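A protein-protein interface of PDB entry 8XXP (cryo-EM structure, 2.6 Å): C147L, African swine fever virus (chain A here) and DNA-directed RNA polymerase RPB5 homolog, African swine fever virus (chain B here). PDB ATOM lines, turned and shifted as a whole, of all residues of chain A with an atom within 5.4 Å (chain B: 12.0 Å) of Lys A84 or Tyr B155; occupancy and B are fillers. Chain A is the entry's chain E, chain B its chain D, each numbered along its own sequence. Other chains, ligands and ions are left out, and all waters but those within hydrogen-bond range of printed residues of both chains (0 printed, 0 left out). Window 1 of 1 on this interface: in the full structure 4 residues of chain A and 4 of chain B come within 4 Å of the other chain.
Among the printed residues, pairs that only touch across the chains: Ile A26 with Arg B153 (3.6 Å), Ile A83 with Tyr B155 (3.2 Å), Lys A84 with Tyr B155 (3.6 Å) and Ile A92 with Tyr B155 (3.5 Å).
Of the 19 printed residues of chain B, 4 touch a printed residue of chain A. Printed residues of chain B that touch a printed residue of chain A: Arg B153, Tyr B155, Gln B157 and Asp B160. Hydrophobic or aromatic side chains of chain B within 4 Å of the printed part of chain A: Tyr B155. Of the 11 printed residues of chain A, 4 touch a printed residue of chain B. Among the printed residues, Asp or Glu carboxylates within 4 Å of a Lys or Arg side-chain nitrogen of the other chain: Lys A84 with Asp B160 (3.9 Å).
The backbone NH (N) of Gln B157 is in hydrogen-bond range of the side-chain carboxylate (OD2) of Asp B160 (3.3 Å). The backbone NH (N) of Ile A83 is in hydrogen-bond range of the backbone carbonyl oxygen (O) of Ile A92 (2.9 Å). O of Lys A84 is in hydrogen-bond range of N of Ile A92, 2.8 Å away.
Printed residues of chain B within 4 Å of Lys A84: Tyr B155 (3.6 Å), Gln B157 (3.4 Å) and Asp B160 (3.9 Å). Tyr B155 touches just these residues of chain A: Ile A83 (3.2 Å), Lys A84 (3.6 Å) and Ile A92 (3.5 Å). No residue of chain B comes within 4 Å of Cys A82. Ile A83 touches just one residue of chain B: Tyr B155. No residue of chain B comes within 4 Å of Val A85. No residue of chain B comes within 4 Å of Thr A86. No residue of chain B comes within 4 Å of Lys A91. No residue of chain B comes within 4 Å of Val A93. Of the printed residues of chain A, Asp B160 touches Lys A84. Of the printed residues of chain B, Ile A26 touches Arg B153. Of the printed residues of chain A, Arg B153 touches Ile A26. The nearest residue of chain B that does not touch Lys A84 is Leu B156 (4.9 Å). The nearest residue of chain A that does not touch Tyr B155 is Ile A20 (4.2 Å). The nearest printed residue of chain A that does not touch Arg B153 is Ile A83 (6.7 Å).
OE1 of Gln B157 sits at hydrogen-bond distance from NZ of Lys A84, at 3.4 Å. NZ of Lys A84 lies within salt-bridge range of OD2 of Asp B160, at 3.9 Å.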
ATOM      1  N   ILE A  20      23.777  -9.943   8.591  1.00  0.00           N
ATOM      2  CA  ILE A  20      24.225  -8.826   9.425  1.00  0.00           C
ATOM      3  C   ILE A  20      24.212  -9.259  10.884  1.00  0.00           C
ATOM      4  O   ILE A  20      23.229  -9.880  11.332  1.00  0.00           O
ATOM      5  CB  ILE A  20      23.323  -7.604   9.199  1.00  0.00           C
ATOM      6  CG1 ILE A  20      23.579  -7.014   7.819  1.00  0.00           C
ATOM      7  CG2 ILE A  20      23.547  -6.559  10.260  1.00  0.00           C
ATOM      8  CD1 ILE A  20      22.493  -6.098   7.347  1.00  0.00           C
ATOM      9  N   ILE A  26      19.452  -2.753  12.038  1.00  0.00           N
ATOM     10  CA  ILE A  26      18.795  -1.461  12.195  1.00  0.00           C
ATOM     11  C   ILE A  26      17.335  -1.485  11.779  1.00  0.00           C
ATOM     12  O   ILE A  26      16.664  -0.458  11.877  1.00  0.00           O
ATOM     13  CB  ILE A  26      19.544  -0.348  11.437  1.00  0.00           C
ATOM     14  CG1 ILE A  26      19.696  -0.708   9.964  1.00  0.00           C
ATOM     15  CG2 ILE A  26      20.893  -0.090  12.073  1.00  0.00           C
ATOM     16  CD1 ILE A  26      20.703   0.135   9.247  1.00  0.00           C
ATOM     17  N   CYS A  82      15.942  -8.940   3.440  1.00  0.00           N
ATOM     18  CA  CYS A  82      17.006  -8.652   2.490  1.00  0.00           C
ATOM     19  C   CYS A  82      17.105  -7.150   2.303  1.00  0.00           C
ATOM     20  O   CYS A  82      16.205  -6.525   1.735  1.00  0.00           O
ATOM     21  CB  CYS A  82      16.752  -9.341   1.156  1.00  0.00           C
ATOM     22  SG  CYS A  82      18.002  -8.963  -0.091  1.00  0.00           S
ATOM     23  N   ILE A  83      18.199  -6.568   2.776  1.00  0.00           N
ATOM     24  CA  ILE A  83      18.360  -5.122   2.747  1.00  0.00           C
ATOM     25  C   ILE A  83      19.231  -4.641   1.598  1.00  0.00           C
ATOM     26  O   ILE A  83      19.151  -3.455   1.241  1.00  0.00           O
ATOM     27  CB  ILE A  83      18.901  -4.596   4.093  1.00  0.00           C
ATOM     28  CG1 ILE A  83      20.357  -4.969   4.251  1.00  0.00           C
ATOM     29  CG2 ILE A  83      18.106  -5.154   5.255  1.00  0.00           C
ATOM     30  CD1 ILE A  83      21.248  -3.835   4.056  1.00  0.00           C
ATOM     31  N   LYS A  84      20.032  -5.509   0.990  1.00  0.00           N
ATOM     32  CA  LYS A  84      20.939  -5.086  -0.065  1.00  0.00           C
ATOM     33  C   LYS A  84      21.354  -6.291  -0.890  1.00  0.00           C
ATOM     34  O   LYS A  84      21.624  -7.360  -0.342  1.00  0.00           O
ATOM     35  CB  LYS A  84      22.178  -4.399   0.519  1.00  0.00           C
ATOM     36  CG  LYS A  84      23.048  -3.681  -0.485  1.00  0.00           C
ATOM     37  CD  LYS A  84      22.255  -2.776  -1.393  1.00  0.00           C
ATOM     38  CE  LYS A  84      23.189  -1.971  -2.281  1.00  0.00           C
ATOM     39  NZ  LYS A  84      22.456  -1.037  -3.174  1.00  0.00           N
ATOM     40  N   VAL A  85      21.392  -6.113  -2.207  1.00  0.00           N
ATOM     41  CA  VAL A  85      22.016  -7.066  -3.115  1.00  0.00           C
ATOM     42  C   VAL A  85      23.178  -6.344  -3.775  1.00  0.00           C
ATOM     43  O   VAL A  85      22.977  -5.499  -4.656  1.00  0.00           O
ATOM     44  CB  VAL A  85      21.031  -7.610  -4.159  1.00  0.00           C
ATOM     45  CG1 VAL A  85      21.782  -8.275  -5.291  1.00  0.00           C
ATOM     46  CG2 VAL A  85      20.064  -8.588  -3.520  1.00  0.00           C
ATOM     47  N   THR A  86      24.380  -6.655  -3.332  1.00  0.00           N
ATOM     48  CA  THR A  86      25.701  -6.131  -3.638  1.00  0.00           C
ATOM     49  C   THR A  86      26.153  -6.590  -5.023  1.00  0.00           C
ATOM     50  O   THR A  86      25.938  -7.746  -5.395  1.00  0.00           O
ATOM     51  CB  THR A  86      26.695  -6.590  -2.580  1.00  0.00           C
ATOM     52  OG1 THR A  86      26.339  -6.017  -1.318  1.00  0.00           O
ATOM     53  CG2 THR A  86      28.082  -6.180  -2.925  1.00  0.00           C
ATOM     54  N   GLN A  90      26.942 -10.320  -3.035  1.00  0.00           N
ATOM     55  CA  GLN A  90      26.614 -10.509  -1.632  1.00  0.00           C
ATOM     56  C   GLN A  90      25.149 -10.166  -1.432  1.00  0.00           C
ATOM     57  O   GLN A  90      24.694  -9.106  -1.870  1.00  0.00           O
ATOM     58  CB  GLN A  90      27.488  -9.627  -0.744  1.00  0.00           C
ATOM     59  CG  GLN A  90      28.970  -9.739  -1.034  1.00  0.00           C
ATOM     60  CD  GLN A  90      29.785 -10.071   0.195  1.00  0.00           C
ATOM     61  OE1 GLN A  90      29.917 -11.233   0.572  1.00  0.00           O
ATOM     62  NE2 GLN A  90      30.315  -9.045   0.844  1.00  0.00           N
ATOM     63  N   LYS A  91      24.408 -11.062  -0.800  1.00  0.00           N
ATOM     64  CA  LYS A  91      23.026 -10.793  -0.425  1.00  0.00           C
ATOM     65  C   LYS A  91      23.037 -10.454   1.056  1.00  0.00           C
ATOM     66  O   LYS A  91      23.122 -11.339   1.907  1.00  0.00           O
ATOM     67  CB  LYS A  91      22.120 -11.978  -0.734  1.00  0.00           C
ATOM     68  CG  LYS A  91      20.648 -11.663  -0.603  1.00  0.00           C
ATOM     69  CD  LYS A  91      19.797 -12.851  -0.983  1.00  0.00           C
ATOM     70  CE  LYS A  91      18.329 -12.579  -0.735  1.00  0.00           C
ATOM     71  NZ  LYS A  91      17.776 -11.638  -1.738  1.00  0.00           N
ATOM     72  N   ILE A  92      22.966  -9.167   1.361  1.00  0.00           N
ATOM     73  CA  ILE A  92      23.054  -8.687   2.732  1.00  0.00           C
ATOM     74  C   ILE A  92      21.654  -8.671   3.324  1.00  0.00           C
ATOM     75  O   ILE A  92      20.780  -7.941   2.848  1.00  0.00           O
ATOM     76  CB  ILE A  92      23.704  -7.299   2.788  1.00  0.00           C
ATOM     77  CG1 ILE A  92      24.962  -7.290   1.920  1.00  0.00           C
ATOM     78  CG2 ILE A  92      24.046  -6.932   4.204  1.00  0.00           C
ATOM     79  CD1 ILE A  92      25.703  -5.988   1.930  1.00  0.00           C
ATOM     80  N   VAL A  93      21.437  -9.482   4.358  1.00  0.00           N
ATOM     81  CA  VAL A  93      20.123  -9.644   4.957  1.00  0.00           C
ATOM     82  C   VAL A  93      20.229  -9.482   6.464  1.00  0.00           C
ATOM     83  O   VAL A  93      21.276  -9.708   7.071  1.00  0.00           O
ATOM     84  CB  VAL A  93      19.481 -11.011   4.623  1.00  0.00           C
ATOM     85  CG1 VAL A  93      19.455 -11.249   3.128  1.00  0.00           C
ATOM     86  CG2 VAL A  93      20.206 -12.132   5.339  1.00  0.00           C
ATOM     87  N   GLU B 146      31.077  12.681   5.434  1.00  0.00           N
ATOM     88  CA  GLU B 146      29.722  12.618   5.969  1.00  0.00           C
ATOM     89  C   GLU B 146      28.796  11.882   5.016  1.00  0.00           C
ATOM     90  O   GLU B 146      27.980  11.057   5.438  1.00  0.00           O
ATOM     91  CB  GLU B 146      29.193  14.025   6.236  1.00  0.00           C
ATOM     92  CG  GLU B 146      29.953  14.806   7.287  1.00  0.00           C
ATOM     93  CD  GLU B 146      29.693  16.298   7.199  1.00  0.00           C
ATOM     94  OE1 GLU B 146      28.544  16.720   7.444  1.00  0.00           O
ATOM     95  OE2 GLU B 146      30.636  17.052   6.881  1.00  0.00           O
ATOM     96  N   ALA B 147      28.913  12.171   3.722  1.00  0.00           N
ATOM     97  CA  ALA B 147      28.114  11.466   2.731  1.00  0.00           C
ATOM     98  C   ALA B 147      28.453   9.985   2.707  1.00  0.00           C
ATOM     99  O   ALA B 147      27.564   9.141   2.582  1.00  0.00           O
ATOM    100  CB  ALA B 147      28.326  12.086   1.355  1.00  0.00           C
ATOM    101  N   GLN B 148      29.736   9.649   2.820  1.00  0.00           N
ATOM    102  CA  GLN B 148      30.135   8.250   2.795  1.00  0.00           C
ATOM    103  C   GLN B 148      29.587   7.496   3.995  1.00  0.00           C
ATOM    104  O   GLN B 148      29.111   6.368   3.854  1.00  0.00           O
ATOM    105  CB  GLN B 148      31.656   8.139   2.740  1.00  0.00           C
ATOM    106  CG  GLN B 148      32.166   6.784   2.281  1.00  0.00           C
ATOM    107  CD  GLN B 148      31.252   6.118   1.272  1.00  0.00           C
ATOM    108  OE1 GLN B 148      30.696   5.048   1.528  1.00  0.00           O
ATOM    109  NE2 GLN B 148      31.109   6.737   0.106  1.00  0.00           N
ATOM    110  N   GLU B 149      29.638   8.096   5.183  1.00  0.00           N
ATOM    111  CA  GLU B 149      29.106   7.406   6.353  1.00  0.00           C
ATOM    112  C   GLU B 149      27.585   7.313   6.296  1.00  0.00           C
ATOM    113  O   GLU B 149      27.006   6.304   6.718  1.00  0.00           O
ATOM    114  CB  GLU B 149      29.573   8.088   7.640  1.00  0.00           C
ATOM    115  CG  GLU B 149      29.081   9.497   7.844  1.00  0.00           C
ATOM    116  CD  GLU B 149      28.009   9.594   8.911  1.00  0.00           C
ATOM    117  OE1 GLU B 149      27.982   8.721   9.803  1.00  0.00           O
ATOM    118  OE2 GLU B 149      27.192  10.538   8.854  1.00  0.00           O
ATOM    119  N   PHE B 150      26.921   8.342   5.761  1.00  0.00           N
ATOM    120  CA  PHE B 150      25.474   8.280   5.590  1.00  0.00           C
ATOM    121  C   PHE B 150      25.082   7.181   4.614  1.00  0.00           C
ATOM    122  O   PHE B 150      24.124   6.440   4.854  1.00  0.00           O
ATOM    123  CB  PHE B 150      24.948   9.633   5.116  1.00  0.00           C
ATOM    124  CG  PHE B 150      23.572   9.579   4.516  1.00  0.00           C
ATOM    125  CD1 PHE B 150      22.453   9.541   5.324  1.00  0.00           C
ATOM    126  CD2 PHE B 150      23.398   9.577   3.144  1.00  0.00           C
ATOM    127  CE1 PHE B 150      21.194   9.496   4.775  1.00  0.00           C
ATOM    128  CE2 PHE B 150      22.139   9.526   2.594  1.00  0.00           C
ATOM    129  CZ  PHE B 150      21.037   9.488   3.409  1.00  0.00           C
ATOM    130  N   LEU B 151      25.810   7.059   3.504  1.00  0.00           N
ATOM    131  CA  LEU B 151      25.498   6.036   2.515  1.00  0.00           C
ATOM    132  C   LEU B 151      25.845   4.647   3.027  1.00  0.00           C
ATOM    133  O   LEU B 151      25.178   3.668   2.680  1.00  0.00           O
ATOM    134  CB  LEU B 151      26.235   6.326   1.211  1.00  0.00           C
ATOM    135  CG  LEU B 151      25.775   7.517   0.376  1.00  0.00           C
ATOM    136  CD1 LEU B 151      26.710   7.713  -0.786  1.00  0.00           C
ATOM    137  CD2 LEU B 151      24.363   7.314  -0.111  1.00  0.00           C
ATOM    138  N   GLY B 152      26.903   4.535   3.828  1.00  0.00           N
ATOM    139  CA  GLY B 152      27.244   3.250   4.406  1.00  0.00           C
ATOM    140  C   GLY B 152      26.216   2.777   5.408  1.00  0.00           C
ATOM    141  O   GLY B 152      25.873   1.593   5.446  1.00  0.00           O
ATOM    142  N   ARG B 153      25.712   3.692   6.238  1.00  0.00           N
ATOM    143  CA  ARG B 153      24.660   3.326   7.175  1.00  0.00           C
ATOM    144  C   ARG B 153      23.371   2.953   6.457  1.00  0.00           C
ATOM    145  O   ARG B 153      22.629   2.086   6.927  1.00  0.00           O
ATOM    146  CB  ARG B 153      24.414   4.469   8.153  1.00  0.00           C
ATOM    147  CG  ARG B 153      23.529   4.110   9.318  1.00  0.00           C
ATOM    148  CD  ARG B 153      22.165   4.746   9.194  1.00  0.00           C
ATOM    149  NE  ARG B 153      21.235   4.205  10.175  1.00  0.00           N
ATOM    150  CZ  ARG B 153      19.921   4.169  10.018  1.00  0.00           C
ATOM    151  NH1 ARG B 153      19.344   4.663   8.937  1.00  0.00           N
ATOM    152  NH2 ARG B 153      19.168   3.626  10.966  1.00  0.00           N
ATOM    153  N   GLU B 154      23.091   3.590   5.330  1.00  0.00           N
ATOM    154  CA  GLU B 154      21.862   3.374   4.583  1.00  0.00           C
ATOM    155  C   GLU B 154      21.999   2.317   3.502  1.00  0.00           C
ATOM    156  O   GLU B 154      21.000   1.994   2.853  1.00  0.00           O
ATOM    157  CB  GLU B 154      21.401   4.684   3.945  1.00  0.00           C
ATOM    158  CG  GLU B 154      21.061   5.776   4.928  1.00  0.00           C
ATOM    159  CD  GLU B 154      19.664   5.651   5.474  1.00  0.00           C
ATOM    160  OE1 GLU B 154      18.709   5.713   4.674  1.00  0.00           O
ATOM    161  OE2 GLU B 154      19.520   5.497   6.703  1.00  0.00           O
ATOM    162  N   TYR B 155      23.199   1.781   3.288  1.00  0.00           N
ATOM    163  CA  TYR B 155      23.452   0.787   2.247  1.00  0.00           C
ATOM    164  C   TYR B 155      23.022   1.299   0.877  1.00  0.00           C
ATOM    165  O   TYR B 155      22.354   0.609   0.106  1.00  0.00           O
ATOM    166  CB  TYR B 155      22.759  -0.530   2.580  1.00  0.00           C
ATOM    167  CG  TYR B 155      23.560  -1.433   3.477  1.00  0.00           C
ATOM    168  CD1 TYR B 155      24.570  -2.224   2.964  1.00  0.00           C
ATOM    169  CD2 TYR B 155      23.329  -1.470   4.840  1.00  0.00           C
ATOM    170  CE1 TYR B 155      25.305  -3.050   3.777  1.00  0.00           C
ATOM    171  CE2 TYR B 155      24.055  -2.297   5.658  1.00  0.00           C
ATOM    172  CZ  TYR B 155      25.044  -3.082   5.122  1.00  0.00           C
ATOM    173  OH  TYR B 155      25.780  -3.903   5.937  1.00  0.00           O
ATOM    174  N   LEU B 156      23.415   2.528   0.570  1.00  0.00           N
ATOM    175  CA  LEU B 156      23.029   3.184  -0.667  1.00  0.00           C
ATOM    176  C   LEU B 156      24.260   3.562  -1.471  1.00  0.00           C
ATOM    177  O   LEU B 156      25.302   3.908  -0.908  1.00  0.00           O
ATOM    178  CB  LEU B 156      22.204   4.442  -0.398  1.00  0.00           C
ATOM    179  CG  LEU B 156      20.804   4.291   0.181  1.00  0.00           C
ATOM    180  CD1 LEU B 156      20.307   5.632   0.640  1.00  0.00           C
ATOM    181  CD2 LEU B 156      19.868   3.710  -0.843  1.00  0.00           C
ATOM    182  N   GLN B 157      24.135   3.484  -2.782  1.00  0.00           N
ATOM    183  CA  GLN B 157      25.089   4.103  -3.675  1.00  0.00           C
ATOM    184  C   GLN B 157      24.703   5.560  -3.888  1.00  0.00           C
ATOM    185  O   GLN B 157      23.555   5.940  -3.667  1.00  0.00           O
ATOM    186  CB  GLN B 157      25.122   3.359  -5.004  1.00  0.00           C
ATOM    187  CG  GLN B 157      26.344   2.496  -5.171  1.00  0.00           C
ATOM    188  CD  GLN B 157      26.334   1.315  -4.232  1.00  0.00           C
ATOM    189  OE1 GLN B 157      25.277   0.779  -3.907  1.00  0.00           O
ATOM    190  NE2 GLN B 157      27.511   0.907  -3.778  1.00  0.00           N
ATOM    191  N   PRO B 158      25.648   6.403  -4.303  1.00  0.00           N
ATOM    192  CA  PRO B 158      25.289   7.799  -4.581  1.00  0.00           C
ATOM    193  C   PRO B 158      24.208   7.938  -5.633  1.00  0.00           C
ATOM    194  O   PRO B 158      23.459   8.918  -5.614  1.00  0.00           O
ATOM    195  CB  PRO B 158      26.614   8.410  -5.047  1.00  0.00           C
ATOM    196  CG  PRO B 158      27.647   7.576  -4.410  1.00  0.00           C
ATOM    197  CD  PRO B 158      27.100   6.186  -4.371  1.00  0.00           C
ATOM    198  N   GLN B 159      24.098   6.976  -6.544  1.00  0.00           N
ATOM    199  CA  GLN B 159      23.111   7.020  -7.611  1.00  0.00           C
ATOM    200  C   GLN B 159      21.712   6.650  -7.147  1.00  0.00           C
ATOM    201  O   GLN B 159      20.750   6.893  -7.881  1.00  0.00           O
ATOM    202  CB  GLN B 159      23.542   6.093  -8.747  1.00  0.00           C
ATOM    203  CG  GLN B 159      24.789   6.564  -9.467  1.00  0.00           C
ATOM    204  CD  GLN B 159      26.055   6.215  -8.719  1.00  0.00           C
ATOM    205  OE1 GLN B 159      26.070   5.296  -7.904  1.00  0.00           O
ATOM    206  NE2 GLN B 159      27.121   6.963  -8.972  1.00  0.00           N
ATOM    207  N   ASP B 160      21.574   6.058  -5.961  1.00  0.00           N
ATOM    208  CA  ASP B 160      20.260   5.779  -5.403  1.00  0.00           C
ATOM    209  C   ASP B 160      19.597   7.015  -4.824  1.00  0.00           C
ATOM    210  O   ASP B 160      18.373   7.030  -4.669  1.00  0.00           O
ATOM    211  CB  ASP B 160      20.367   4.717  -4.310  1.00  0.00           C
ATOM    212  CG  ASP B 160      20.827   3.383  -4.839  1.00  0.00           C
ATOM    213  OD1 ASP B 160      20.757   3.169  -6.065  1.00  0.00           O
ATOM    214  OD2 ASP B 160      21.261   2.545  -4.026  1.00  0.00           O
ATOM    215  N   LEU B 161      20.369   8.042  -4.496  1.00  0.00           N
ATOM    216  CA  LEU B 161      19.822   9.230  -3.871  1.00  0.00           C
ATOM    217  C   LEU B 161      18.982  10.022  -4.860  1.00  0.00           C
ATOM    218  O   LEU B 161      19.099   9.875  -6.078  1.00  0.00           O
ATOM    219  CB  LEU B 161      20.938  10.120  -3.332  1.00  0.00           C
ATOM    220  CG  LEU B 161      21.793   9.575  -2.199  1.00  0.00           C
ATOM    221  CD1 LEU B 161      22.674  10.675  -1.667  1.00  0.00           C
ATOM    222  CD2 LEU B 161      20.916   9.016  -1.103  1.00  0.00           C
ATOM    223  N   MET B 162      18.116  10.870  -4.316  1.00  0.00           N
ATOM    224  CA  MET B 162      17.434  11.853  -5.139  1.00  0.00           C
ATOM    225  C   MET B 162      18.461  12.799  -5.731  1.00  0.00           C
ATOM    226  O   MET B 162      19.493  13.082  -5.121  1.00  0.00           O
ATOM    227  CB  MET B 162      16.409  12.625  -4.314  1.00  0.00           C
ATOM    228  CG  MET B 162      15.229  11.788  -3.881  1.00  0.00           C
ATOM    229  SD  MET B 162      15.182  11.521  -2.102  1.00  0.00           S
ATOM    230  CE  MET B 162      14.416  13.041  -1.569  1.00  0.00           C
ATOM    231  N   PHE B 181      27.397  16.150  -2.616  1.00  0.00           N
ATOM    232  CA  PHE B 181      26.146  15.888  -1.927  1.00  0.00           C
ATOM    233  C   PHE B 181      25.705  17.157  -1.222  1.00  0.00           C
ATOM    234  O   PHE B 181      26.514  17.816  -0.566  1.00  0.00           O
ATOM    235  CB  PHE B 181      26.303  14.750  -0.923  1.00  0.00           C
ATOM    236  CG  PHE B 181      26.729  13.457  -1.538  1.00  0.00           C
ATOM    237  CD1 PHE B 181      28.049  13.234  -1.872  1.00  0.00           C
ATOM    238  CD2 PHE B 181      25.808  12.462  -1.787  1.00  0.00           C
ATOM    239  CE1 PHE B 181      28.435  12.053  -2.436  1.00  0.00           C
ATOM    240  CE2 PHE B 181      26.195  11.277  -2.351  1.00  0.00           C
ATOM    241  CZ  PHE B 181      27.509  11.073  -2.675  1.00  0.00           C
ATOM    242  N   ILE B 197      19.171  14.328   1.544  1.00  0.00           N
ATOM    243  CA  ILE B 197      20.456  14.513   0.889  1.00  0.00           C
ATOM    244  C   ILE B 197      20.265  14.217  -0.589  1.00  0.00           C
ATOM    245  O   ILE B 197      19.758  13.151  -0.950  1.00  0.00           O
ATOM    246  CB  ILE B 197      21.540  13.613   1.506  1.00  0.00           C
ATOM    247  CG1 ILE B 197      21.793  14.027   2.955  1.00  0.00           C
ATOM    248  CG2 ILE B 197      22.819  13.690   0.703  1.00  0.00           C
ATOM    249  CD1 ILE B 197      22.629  13.057   3.733  1.00  0.00           C
